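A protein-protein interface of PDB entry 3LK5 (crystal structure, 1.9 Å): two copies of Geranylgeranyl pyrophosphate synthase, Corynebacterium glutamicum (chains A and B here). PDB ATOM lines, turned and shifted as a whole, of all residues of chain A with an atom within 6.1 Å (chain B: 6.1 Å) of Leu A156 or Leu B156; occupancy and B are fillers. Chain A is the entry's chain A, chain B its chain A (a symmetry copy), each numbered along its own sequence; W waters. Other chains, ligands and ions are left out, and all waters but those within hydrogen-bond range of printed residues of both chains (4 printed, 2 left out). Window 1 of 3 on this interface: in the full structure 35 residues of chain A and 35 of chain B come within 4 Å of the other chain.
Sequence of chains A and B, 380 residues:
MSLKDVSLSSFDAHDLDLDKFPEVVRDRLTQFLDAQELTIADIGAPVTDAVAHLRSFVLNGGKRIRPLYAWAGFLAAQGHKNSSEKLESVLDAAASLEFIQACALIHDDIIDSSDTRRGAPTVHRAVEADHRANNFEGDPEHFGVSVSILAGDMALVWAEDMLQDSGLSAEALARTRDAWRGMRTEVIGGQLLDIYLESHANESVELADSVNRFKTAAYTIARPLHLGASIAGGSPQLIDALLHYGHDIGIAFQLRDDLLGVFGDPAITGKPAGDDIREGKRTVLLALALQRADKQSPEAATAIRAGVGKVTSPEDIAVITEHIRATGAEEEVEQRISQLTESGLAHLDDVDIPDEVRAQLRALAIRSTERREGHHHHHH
Hydrophobic or aromatic side chains of chain B that line the printed part of chain A: Met B154, Leu B156, Val B157 and Ile B188. Hydrophobic or aromatic side chains of chain A that line the printed part of chain B: Met A154, Leu A156, Val A157 and Ile A188. Among the printed residues, Asp or Glu carboxylates within 4 Å of a Lys or Arg side-chain nitrogen of the other chain: Asp A161 with Arg B184 and Arg A184 with Asp B161.
Asp A153 touches its own counterpart, Asp B153. Leu A156 touches its own counterpart, Leu B156. Glu B160 touches its own counterpart, Glu A160. Glu A160 touches Arg B184, and with the chains exchanged Arg A184 touches Glu B160. Of the 17 pairs that touch across the chains among the printed residues, 17 have their exchanged pair printed and touching as well.
Among the printed residues, pairs that only touch across the chains: Glu A160 with Arg B184, Arg A184 with Glu B160, Asp A153 with Asp B153, Glu A160 with Glu B160, Asp A153 with Ile B188, Ile A188 with Asp B153, Met A154 with Ile B188, Ile A188 with Met B154, Ile A188 with Val B157, Val A157 with Ile B188, Leu A156 with Val B157, Val A157 with Leu B156 and Leu A156 with Leu B156.
NE1 of Trp B158 sits close to SD of Met B154, 3.8 Å away. NE1 of Trp A158 sits close to SD of Met A154. OE2 of Glu B160 lies within salt-bridge range of NE of Arg B184, 2.9 Å away. The side-chain carboxylate (OE2) of Glu A160 lies within salt-bridge range of the guanidinium group (NE) of Arg A184.
Water W4 lies within hydrogen-bond range of the side-chain carboxylate of Asp A161 and the guanidinium group of Arg B184. Water W2 bridges OD2 of Asp B161 and NH1 of Arg A184. Water W1 lies within hydrogen-bond range of NH2 of Arg A184, OD1 of Asp B161 and OE1 of Glu A160. Water W3 lies within hydrogen-bond range of NH2 of Arg B184 (3.2 Å), OD1 of Asp A161 (3.4 Å) and OE1 of Glu B160 (3.5 Å).
Of chain B, only Leu B156 (3.8 Å) and Val B157 (3.8 Å) come within 4 Å of Leu A156. Leu B156 touches two residues of chain A. Printed residues of chain A within 4 Å of Glu B160: Glu A160 (3.6 Å) and Arg A184 (3.5 Å). Of the printed residues of chain B, Glu A160 touches Glu B160 (3.6 Å) and Arg B184 (3.5 Å). Of the printed residues of chain B, Asp A153 touches Asp B153 (3.6 Å) and Ile B188 (3.7 Å). Of the printed residues of chain B, Asp A161 touches Arg B184 (2.9 Å). Ala A159 touches none of the printed residues of chain B. Gly A152 touches none of the printed residues of chain B.
NH2 of Arg A184 sits at hydrogen-bond distance from O of Val B157 (3.1 Å). The backbone carbonyl oxygen (O) of Val A157 sits at hydrogen-bond distance from the guanidinium group (NH2) of Arg B184 (3.1 Å). OD1 of Asp B161 lies within salt-bridge range of NH1 of Arg A184. The side-chain carboxylate of Asp A161 lies within salt-bridge range of the guanidinium group of Arg B184.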
ATOM      1  N   PHE A  99      14.914   1.301  27.030  1.00  0.00           N
ATOM      2  CA  PHE A  99      13.578   0.772  26.679  1.00  0.00           C
ATOM      3  C   PHE A  99      12.756   0.379  27.902  1.00  0.00           C
ATOM      4  O   PHE A  99      11.530   0.539  27.913  1.00  0.00           O
ATOM      5  CB  PHE A  99      13.704  -0.387  25.694  1.00  0.00           C
ATOM      6  CG  PHE A  99      13.890   0.039  24.284  1.00  0.00           C
ATOM      7  CD1 PHE A  99      12.906   0.780  23.631  1.00  0.00           C
ATOM      8  CD2 PHE A  99      15.017  -0.350  23.582  1.00  0.00           C
ATOM      9  CE1 PHE A  99      13.046   1.140  22.291  1.00  0.00           C
ATOM     10  CE2 PHE A  99      15.172   0.004  22.246  1.00  0.00           C
ATOM     11  CZ  PHE A  99      14.169   0.765  21.607  1.00  0.00           C
ATOM     12  N   ILE A 100      13.416  -0.141  28.932  1.00  0.00           N
ATOM     13  CA  ILE A 100      12.719  -0.416  30.191  1.00  0.00           C
ATOM     14  C   ILE A 100      12.192   0.903  30.707  1.00  0.00           C
ATOM     15  O   ILE A 100      11.022   1.000  31.100  1.00  0.00           O
ATOM     16  CB  ILE A 100      13.630  -1.055  31.242  1.00  0.00           C
ATOM     17  CG1 ILE A 100      14.164  -2.380  30.690  1.00  0.00           C
ATOM     18  CG2 ILE A 100      12.818  -1.323  32.565  1.00  0.00           C
ATOM     19  CD1 ILE A 100      15.026  -3.149  31.700  1.00  0.00           C
ATOM     20  N   CYS A 103       9.156   2.224  28.843  1.00  0.00           N
ATOM     21  CA  CYS A 103       7.912   1.553  29.275  1.00  0.00           C
ATOM     22  C   CYS A 103       7.456   2.108  30.617  1.00  0.00           C
ATOM     23  O   CYS A 103       6.275   2.404  30.804  1.00  0.00           O
ATOM     24  CB  CYS A 103       8.101   0.037  29.406  1.00  0.00           C
ATOM     25  SG  CYS A 103       6.548  -0.833  29.912  1.00  0.00           S
ATOM     26  N   ALA A 151       2.334   0.632  23.351  1.00  0.00           N
ATOM     27  CA  ALA A 151       3.663   1.196  23.018  1.00  0.00           C
ATOM     28  C   ALA A 151       4.646   0.870  24.120  1.00  0.00           C
ATOM     29  O   ALA A 151       5.799   0.493  23.861  1.00  0.00           O
ATOM     30  CB  ALA A 151       3.597   2.725  22.822  1.00  0.00           C
ATOM     31  N   GLY A 152       4.181   1.005  25.353  1.00  0.00           N
ATOM     32  CA  GLY A 152       5.003   0.643  26.524  1.00  0.00           C
ATOM     33  C   GLY A 152       5.352  -0.836  26.477  1.00  0.00           C
ATOM     34  O   GLY A 152       6.479  -1.220  26.757  1.00  0.00           O
ATOM     35  N   ASP A 153       4.390  -1.673  26.100  1.00  0.00           N
ATOM     36  CA  ASP A 153       4.668  -3.114  26.041  1.00  0.00           C
ATOM     37  C   ASP A 153       5.702  -3.416  24.952  1.00  0.00           C
ATOM     38  O   ASP A 153       6.577  -4.256  25.143  1.00  0.00           O
ATOM     39  CB  ASP A 153       3.397  -3.915  25.760  1.00  0.00           C
ATOM     40  CG  ASP A 153       2.385  -3.880  26.908  1.00  0.00           C
ATOM     41  OD1 ASP A 153       2.735  -3.474  28.034  1.00  0.00           O
ATOM     42  OD2 ASP A 153       1.215  -4.334  26.682  1.00  0.00           O
ATOM     43  N   MET A 154       5.594  -2.730  23.812  1.00  0.00           N
ATOM     44  CA  MET A 154       6.597  -2.870  22.753  1.00  0.00           C
ATOM     45  C   MET A 154       8.000  -2.496  23.263  1.00  0.00           C
ATOM     46  O   MET A 154       8.969  -3.201  22.969  1.00  0.00           O
ATOM     47  CB  MET A 154       6.233  -2.044  21.517  1.00  0.00           C
ATOM     48  CG  MET A 154       7.103  -2.369  20.305  1.00  0.00           C
ATOM     49  SD  MET A 154       6.648  -4.094  19.496  1.00  0.00           S
ATOM     50  CE  MET A 154       5.089  -3.468  18.471  1.00  0.00           C
ATOM     51  N   ALA A 155       8.085  -1.403  24.013  1.00  0.00           N
ATOM     52  CA  ALA A 155       9.371  -0.965  24.576  1.00  0.00           C
ATOM     53  C   ALA A 155       9.918  -2.055  25.487  1.00  0.00           C
ATOM     54  O   ALA A 155      11.111  -2.333  25.468  1.00  0.00           O
ATOM     55  CB  ALA A 155       9.210   0.325  25.330  1.00  0.00           C
ATOM     56  N   LEU A 156       9.055  -2.677  26.275  1.00  0.00           N
ATOM     57  CA  LEU A 156       9.551  -3.693  27.206  1.00  0.00           C
ATOM     58  C   LEU A 156      10.062  -4.946  26.504  1.00  0.00           C
ATOM     59  O   LEU A 156      11.125  -5.484  26.884  1.00  0.00           O
ATOM     60  CB  LEU A 156       8.483  -4.004  28.293  1.00  0.00           C
ATOM     61  CG  LEU A 156       8.865  -4.996  29.394  1.00  0.00           C
ATOM     62  CD1 LEU A 156      10.133  -4.528  30.180  1.00  0.00           C
ATOM     63  CD2 LEU A 156       7.655  -5.092  30.369  1.00  0.00           C
ATOM     64  N   VAL A 157       9.347  -5.414  25.477  1.00  0.00           N
ATOM     65  CA  VAL A 157       9.837  -6.553  24.694  1.00  0.00           C
ATOM     66  C   VAL A 157      11.118  -6.195  23.925  1.00  0.00           C
ATOM     67  O   VAL A 157      12.028  -7.013  23.825  1.00  0.00           O
ATOM     68  CB  VAL A 157       8.746  -7.275  23.773  1.00  0.00           C
ATOM     69  CG1 VAL A 157       7.556  -7.752  24.625  1.00  0.00           C
ATOM     70  CG2 VAL A 157       8.312  -6.466  22.655  1.00  0.00           C
ATOM     71  N   TRP A 158      11.219  -4.962  23.479  1.00  0.00           N
ATOM     72  CA  TRP A 158      12.444  -4.567  22.762  1.00  0.00           C
ATOM     73  C   TRP A 158      13.651  -4.380  23.703  1.00  0.00           C
ATOM     74  O   TRP A 158      14.785  -4.550  23.266  1.00  0.00           O
ATOM     75  CB  TRP A 158      12.185  -3.286  21.952  1.00  0.00           C
ATOM     76  CG  TRP A 158      11.405  -3.622  20.690  1.00  0.00           C
ATOM     77  CD1 TRP A 158      11.088  -4.878  20.211  1.00  0.00           C
ATOM     78  CD2 TRP A 158      10.905  -2.684  19.737  1.00  0.00           C
ATOM     79  NE1 TRP A 158      10.352  -4.758  19.015  1.00  0.00           N
ATOM     80  CE2 TRP A 158      10.262  -3.419  18.711  1.00  0.00           C
ATOM     81  CE3 TRP A 158      10.913  -1.273  19.672  1.00  0.00           C
ATOM     82  CZ2 TRP A 158       9.646  -2.791  17.623  1.00  0.00           C
ATOM     83  CZ3 TRP A 158      10.286  -0.644  18.595  1.00  0.00           C
ATOM     84  CH2 TRP A 158       9.670  -1.407  17.584  1.00  0.00           C
ATOM     85  N   ALA A 159      13.403  -3.981  24.952  1.00  0.00           N
ATOM     86  CA  ALA A 159      14.509  -3.977  25.952  1.00  0.00           C
ATOM     87  C   ALA A 159      15.119  -5.368  26.013  1.00  0.00           C
ATOM     88  O   ALA A 159      16.361  -5.544  25.982  1.00  0.00           O
ATOM     89  CB  ALA A 159      14.023  -3.542  27.352  1.00  0.00           C
ATOM     90  N   GLU A 160      14.248  -6.384  26.117  1.00  0.00           N
ATOM     91  CA  GLU A 160      14.729  -7.758  26.234  1.00  0.00           C
ATOM     92  C   GLU A 160      15.454  -8.145  24.957  1.00  0.00           C
ATOM     93  O   GLU A 160      16.494  -8.767  25.028  1.00  0.00           O
ATOM     94  CB  GLU A 160      13.566  -8.772  26.472  1.00  0.00           C
ATOM     95  CG  GLU A 160      12.596  -8.270  27.536  1.00  0.00           C
ATOM     96  CD  GLU A 160      12.997  -8.557  29.010  1.00  0.00           C
ATOM     97  OE1 GLU A 160      14.145  -9.156  29.193  1.00  0.00           O
ATOM     98  OE2 GLU A 160      12.116  -8.211  29.950  1.00  0.00           O
ATOM     99  N   ASP A 161      14.850  -7.868  23.791  1.00  0.00           N
ATOM    100  CA  ASP A 161      15.496  -8.238  22.498  1.00  0.00           C
ATOM    101  C   ASP A 161      16.856  -7.554  22.381  1.00  0.00           C
ATOM    102  O   ASP A 161      17.800  -8.141  21.865  1.00  0.00           O
ATOM    103  CB  ASP A 161      14.647  -7.753  21.322  1.00  0.00           C
ATOM    104  CG  ASP A 161      13.349  -8.572  21.152  1.00  0.00           C
ATOM    105  OD1 ASP A 161      13.232  -9.706  21.670  1.00  0.00           O
ATOM    106  OD2 ASP A 161      12.429  -8.050  20.518  1.00  0.00           O
ATOM    107  N   ARG A 184      14.154  -6.020  37.101  1.00  0.00           N
ATOM    108  CA  ARG A 184      12.802  -5.886  36.500  1.00  0.00           C
ATOM    109  C   ARG A 184      11.723  -6.264  37.512  1.00  0.00           C
ATOM    110  O   ARG A 184      10.675  -5.628  37.571  1.00  0.00           O
ATOM    111  CB  ARG A 184      12.698  -6.708  35.176  1.00  0.00           C
ATOM    112  CG  ARG A 184      13.455  -5.934  34.056  1.00  0.00           C
ATOM    113  CD  ARG A 184      14.275  -6.874  33.133  1.00  0.00           C
ATOM    114  NE  ARG A 184      13.441  -7.913  32.489  1.00  0.00           N
ATOM    115  CZ  ARG A 184      13.345  -9.188  32.881  1.00  0.00           C
ATOM    116  NH1 ARG A 184      13.979  -9.645  33.975  1.00  0.00           N
ATOM    117  NH2 ARG A 184      12.614 -10.038  32.133  1.00  0.00           N
ATOM    118  N   ILE A 188       9.057  -3.059  39.065  1.00  0.00           N
ATOM    119  CA  ILE A 188       7.609  -3.245  39.004  1.00  0.00           C
ATOM    120  C   ILE A 188       7.047  -3.451  40.429  1.00  0.00           C
ATOM    121  O   ILE A 188       5.976  -2.886  40.781  1.00  0.00           O
ATOM    122  CB  ILE A 188       7.213  -4.390  38.017  1.00  0.00           C
ATOM    123  CG1 ILE A 188       7.838  -4.152  36.632  1.00  0.00           C
ATOM    124  CG2 ILE A 188       5.612  -4.560  37.957  1.00  0.00           C
ATOM    125  CD1 ILE A 188       7.639  -5.276  35.637  1.00  0.00           C
ATOM    126  N   PHE B  99       2.461 -16.609  30.470  1.00  0.00           N
ATOM    127  CA  PHE B  99       2.672 -15.256  31.031  1.00  0.00           C
ATOM    128  C   PHE B  99       2.521 -14.152  29.990  1.00  0.00           C
ATOM    129  O   PHE B  99       2.033 -13.059  30.299  1.00  0.00           O
ATOM    130  CB  PHE B  99       4.020 -15.176  31.741  1.00  0.00           C
ATOM    131  CG  PHE B  99       4.010 -15.730  33.118  1.00  0.00           C
ATOM    132  CD1 PHE B  99       3.206 -15.163  34.105  1.00  0.00           C
ATOM    133  CD2 PHE B  99       4.849 -16.778  33.453  1.00  0.00           C
ATOM    134  CE1 PHE B  99       3.228 -15.642  35.415  1.00  0.00           C
ATOM    135  CE2 PHE B  99       4.879 -17.268  34.754  1.00  0.00           C
ATOM    136  CZ  PHE B  99       4.047 -16.687  35.735  1.00  0.00           C
ATOM    137  N   ILE B 100       2.941 -14.422  28.758  1.00  0.00           N
ATOM    138  CA  ILE B 100       2.707 -13.466  27.673  1.00  0.00           C
ATOM    139  C   ILE B 100       1.211 -13.305  27.535  1.00  0.00           C
ATOM    140  O   ILE B 100       0.705 -12.178  27.455  1.00  0.00           O
ATOM    141  CB  ILE B 100       3.302 -13.928  26.341  1.00  0.00           C
ATOM    142  CG1 ILE B 100       4.814 -14.099  26.510  1.00  0.00           C
ATOM    143  CG2 ILE B 100       3.014 -12.856  25.223  1.00  0.00           C
ATOM    144  CD1 ILE B 100       5.527 -14.482  25.206  1.00  0.00           C
ATOM    145  N   CYS B 103      -0.409 -11.222  30.269  1.00  0.00           N
ATOM    146  CA  CYS B 103      -0.228  -9.775  30.035  1.00  0.00           C
ATOM    147  C   CYS B 103      -1.190  -9.293  28.958  1.00  0.00           C
ATOM    148  O   CYS B 103      -1.834  -8.254  29.112  1.00  0.00           O
ATOM    149  CB  CYS B 103       1.205  -9.444  29.601  1.00  0.00           C
ATOM    150  SG  CYS B 103       1.470  -7.632  29.336  1.00  0.00           S
ATOM    151  N   ALA B 151       0.511  -5.315  36.863  1.00  0.00           N
ATOM    152  CA  ALA B 151       0.429  -6.790  36.963  1.00  0.00           C
ATOM    153  C   ALA B 151       0.739  -7.411  35.620  1.00  0.00           C
ATOM    154  O   ALA B 151       1.468  -8.410  35.527  1.00  0.00           O
ATOM    155  CB  ALA B 151      -0.967  -7.250  37.432  1.00  0.00           C
ATOM    156  N   GLY B 152       0.192  -6.806  34.576  1.00  0.00           N
ATOM    157  CA  GLY B 152       0.477  -7.252  33.198  1.00  0.00           C
ATOM    158  C   GLY B 152       1.962  -7.114  32.903  1.00  0.00           C
ATOM    159  O   GLY B 152       2.562  -7.993  32.300  1.00  0.00           O
ATOM    160  N   ASP B 153       2.568  -6.017  33.346  1.00  0.00           N
ATOM    161  CA  ASP B 153       4.001  -5.827  33.086  1.00  0.00           C
ATOM    162  C   ASP B 153       4.825  -6.884  33.827  1.00  0.00           C
ATOM    163  O   ASP B 153       5.802  -7.398  33.290  1.00  0.00           O
ATOM    164  CB  ASP B 153       4.465  -4.437  33.517  1.00  0.00           C
ATOM    165  CG  ASP B 153       3.881  -3.305  32.667  1.00  0.00           C
ATOM    166  OD1 ASP B 153       3.331  -3.565  31.578  1.00  0.00           O
ATOM    167  OD2 ASP B 153       4.037  -2.109  33.083  1.00  0.00           O
ATOM    168  N   MET B 154       4.427  -7.200  35.062  1.00  0.00           N
ATOM    169  CA  MET B 154       5.084  -8.275  35.810  1.00  0.00           C
ATOM    170  C   MET B 154       5.000  -9.612  35.055  1.00  0.00           C
ATOM    171  O   MET B 154       5.993 -10.342  34.982  1.00  0.00           O
ATOM    172  CB  MET B 154       4.509  -8.414  37.222  1.00  0.00           C
ATOM    173  CG  MET B 154       5.340  -9.331  38.116  1.00  0.00           C
ATOM    174  SD  MET B 154       7.015  -8.499  38.697  1.00  0.00           S
ATOM    175  CE  MET B 154       6.248  -7.424  40.157  1.00  0.00           C
ATOM    176  N   ALA B 155       3.826  -9.909  34.508  1.00  0.00           N
ATOM    177  CA  ALA B 155       3.637 -11.149  33.740  1.00  0.00           C
ATOM    178  C   ALA B 155       4.585 -11.153  32.549  1.00  0.00           C
ATOM    179  O   ALA B 155       5.176 -12.178  32.235  1.00  0.00           O
ATOM    180  CB  ALA B 155       2.211 -11.278  33.282  1.00  0.00           C
ATOM    181  N   LEU B 156       4.740 -10.013  31.894  1.00  0.00           N
ATOM    182  CA  LEU B 156       5.601  -9.989  30.709  1.00  0.00           C
ATOM    183  C   LEU B 156       7.076 -10.188  31.040  1.00  0.00           C
ATOM    184  O   LEU B 156       7.779 -10.940  30.330  1.00  0.00           O
ATOM    185  CB  LEU B 156       5.339  -8.706  29.871  1.00  0.00           C
ATOM    186  CG  LEU B 156       6.106  -8.554  28.555  1.00  0.00           C
ATOM    187  CD1 LEU B 156       5.831  -9.748  27.583  1.00  0.00           C
ATOM    188  CD2 LEU B 156       5.632  -7.227  27.895  1.00  0.00           C
ATOM    189  N   VAL B 157       7.561  -9.551  32.110  1.00  0.00           N
ATOM    190  CA  VAL B 157       8.942  -9.781  32.543  1.00  0.00           C
ATOM    191  C   VAL B 157       9.144 -11.223  33.036  1.00  0.00           C
ATOM    192  O   VAL B 157      10.180 -11.828  32.772  1.00  0.00           O
ATOM    193  CB  VAL B 157       9.536  -8.695  33.557  1.00  0.00           C
ATOM    194  CG1 VAL B 157       9.451  -7.286  32.943  1.00  0.00           C
ATOM    195  CG2 VAL B 157       8.928  -8.743  34.870  1.00  0.00           C
ATOM    196  N   TRP B 158       8.128 -11.788  33.652  1.00  0.00           N
ATOM    197  CA  TRP B 158       8.267 -13.180  34.114  1.00  0.00           C
ATOM    198  C   TRP B 158       8.200 -14.200  32.961  1.00  0.00           C
ATOM    199  O   TRP B 158       8.774 -15.278  33.078  1.00  0.00           O
ATOM    200  CB  TRP B 158       7.196 -13.487  35.173  1.00  0.00           C
ATOM    201  CG  TRP B 158       7.595 -12.873  36.506  1.00  0.00           C
ATOM    202  CD1 TRP B 158       8.793 -12.261  36.821  1.00  0.00           C
ATOM    203  CD2 TRP B 158       6.811 -12.872  37.699  1.00  0.00           C
ATOM    204  NE1 TRP B 158       8.764 -11.822  38.160  1.00  0.00           N
ATOM    205  CE2 TRP B 158       7.563 -12.218  38.704  1.00  0.00           C
ATOM    206  CE3 TRP B 158       5.514 -13.342  38.005  1.00  0.00           C
ATOM    207  CZ2 TRP B 158       7.069 -12.033  40.000  1.00  0.00           C
ATOM    208  CZ3 TRP B 158       5.013 -13.145  39.293  1.00  0.00           C
ATOM    209  CH2 TRP B 158       5.795 -12.504  40.273  1.00  0.00           C
ATOM    210  N   ALA B 159       7.463 -13.879  31.896  1.00  0.00           N
ATOM    211  CA  ALA B 159       7.525 -14.736  30.677  1.00  0.00           C
ATOM    212  C   ALA B 159       8.973 -14.851  30.232  1.00  0.00           C
ATOM    213  O   ALA B 159       9.486 -15.957  29.936  1.00  0.00           O
ATOM    214  CB  ALA B 159       6.652 -14.179  29.531  1.00  0.00           C
ATOM    215  N   GLU B 160       9.657 -13.698  30.163  1.00  0.00           N
ATOM    216  CA  GLU B 160      11.041 -13.687  29.697  1.00  0.00           C
ATOM    217  C   GLU B 160      11.904 -14.462  30.678  1.00  0.00           C
ATOM    218  O   GLU B 160      12.751 -15.220  30.254  1.00  0.00           O
ATOM    219  CB  GLU B 160      11.610 -12.239  29.570  1.00  0.00           C
ATOM    220  CG  GLU B 160      10.623 -11.310  28.872  1.00  0.00           C
ATOM    221  CD  GLU B 160      10.649 -11.336  27.318  1.00  0.00           C
ATOM    222  OE1 GLU B 160      11.479 -12.183  26.766  1.00  0.00           O
ATOM    223  OE2 GLU B 160       9.862 -10.462  26.690  1.00  0.00           O
ATOM    224  N   ASP B 161      11.758 -14.190  31.984  1.00  0.00           N
ATOM    225  CA  ASP B 161      12.588 -14.900  33.001  1.00  0.00           C
ATOM    226  C   ASP B 161      12.351 -16.404  32.909  1.00  0.00           C
ATOM    227  O   ASP B 161      13.280 -17.187  33.075  1.00  0.00           O
ATOM    228  CB  ASP B 161      12.183 -14.467  34.411  1.00  0.00           C
ATOM    229  CG  ASP B 161      12.630 -13.026  34.741  1.00  0.00           C
ATOM    230  OD1 ASP B 161      13.532 -12.467  34.076  1.00  0.00           O
ATOM    231  OD2 ASP B 161      12.043 -12.446  35.656  1.00  0.00           O
ATOM    232  N   ARG B 184       6.676 -11.814  19.754  1.00  0.00           N
ATOM    233  CA  ARG B 184       6.325 -10.702  20.673  1.00  0.00           C
ATOM    234  C   ARG B 184       6.140  -9.399  19.897  1.00  0.00           C
ATOM    235  O   ARG B 184       5.245  -8.615  20.201  1.00  0.00           O
ATOM    236  CB  ARG B 184       7.377 -10.573  21.820  1.00  0.00           C
ATOM    237  CG  ARG B 184       7.130 -11.720  22.844  1.00  0.00           C
ATOM    238  CD  ARG B 184       8.450 -12.346  23.367  1.00  0.00           C
ATOM    239  NE  ARG B 184       9.343 -11.349  24.001  1.00  0.00           N
ATOM    240  CZ  ARG B 184      10.411 -10.785  23.427  1.00  0.00           C
ATOM    241  NH1 ARG B 184      10.750 -11.039  22.151  1.00  0.00           N
ATOM    242  NH2 ARG B 184      11.181  -9.963  24.168  1.00  0.00           N
ATOM    243  N   ILE B 188       2.053  -7.667  19.606  1.00  0.00           N
ATOM    244  CA  ILE B 188       1.843  -6.269  19.976  1.00  0.00           C
ATOM    245  C   ILE B 188       1.542  -5.432  18.713  1.00  0.00           C
ATOM    246  O   ILE B 188       0.638  -4.553  18.729  1.00  0.00           O
ATOM    247  CB  ILE B 188       3.036  -5.707  20.814  1.00  0.00           C
ATOM    248  CG1 ILE B 188       3.315  -6.606  22.031  1.00  0.00           C
ATOM    249  CG2 ILE B 188       2.770  -4.171  21.223  1.00  0.00           C
ATOM    250  CD1 ILE B 188       4.545  -6.236  22.833  1.00  0.00           C
HETATM  251  O   HOH W   1      14.993 -11.942  31.048  1.00  0.00           O
HETATM  252  O   HOH W   2      12.266  -9.981  36.773  1.00  0.00           O
HETATM  253  O   HOH W   3      13.865 -11.762  24.306  1.00  0.00           O
HETATM  254  O   HOH W   4       9.927  -8.850  19.826  1.00  0.00           O
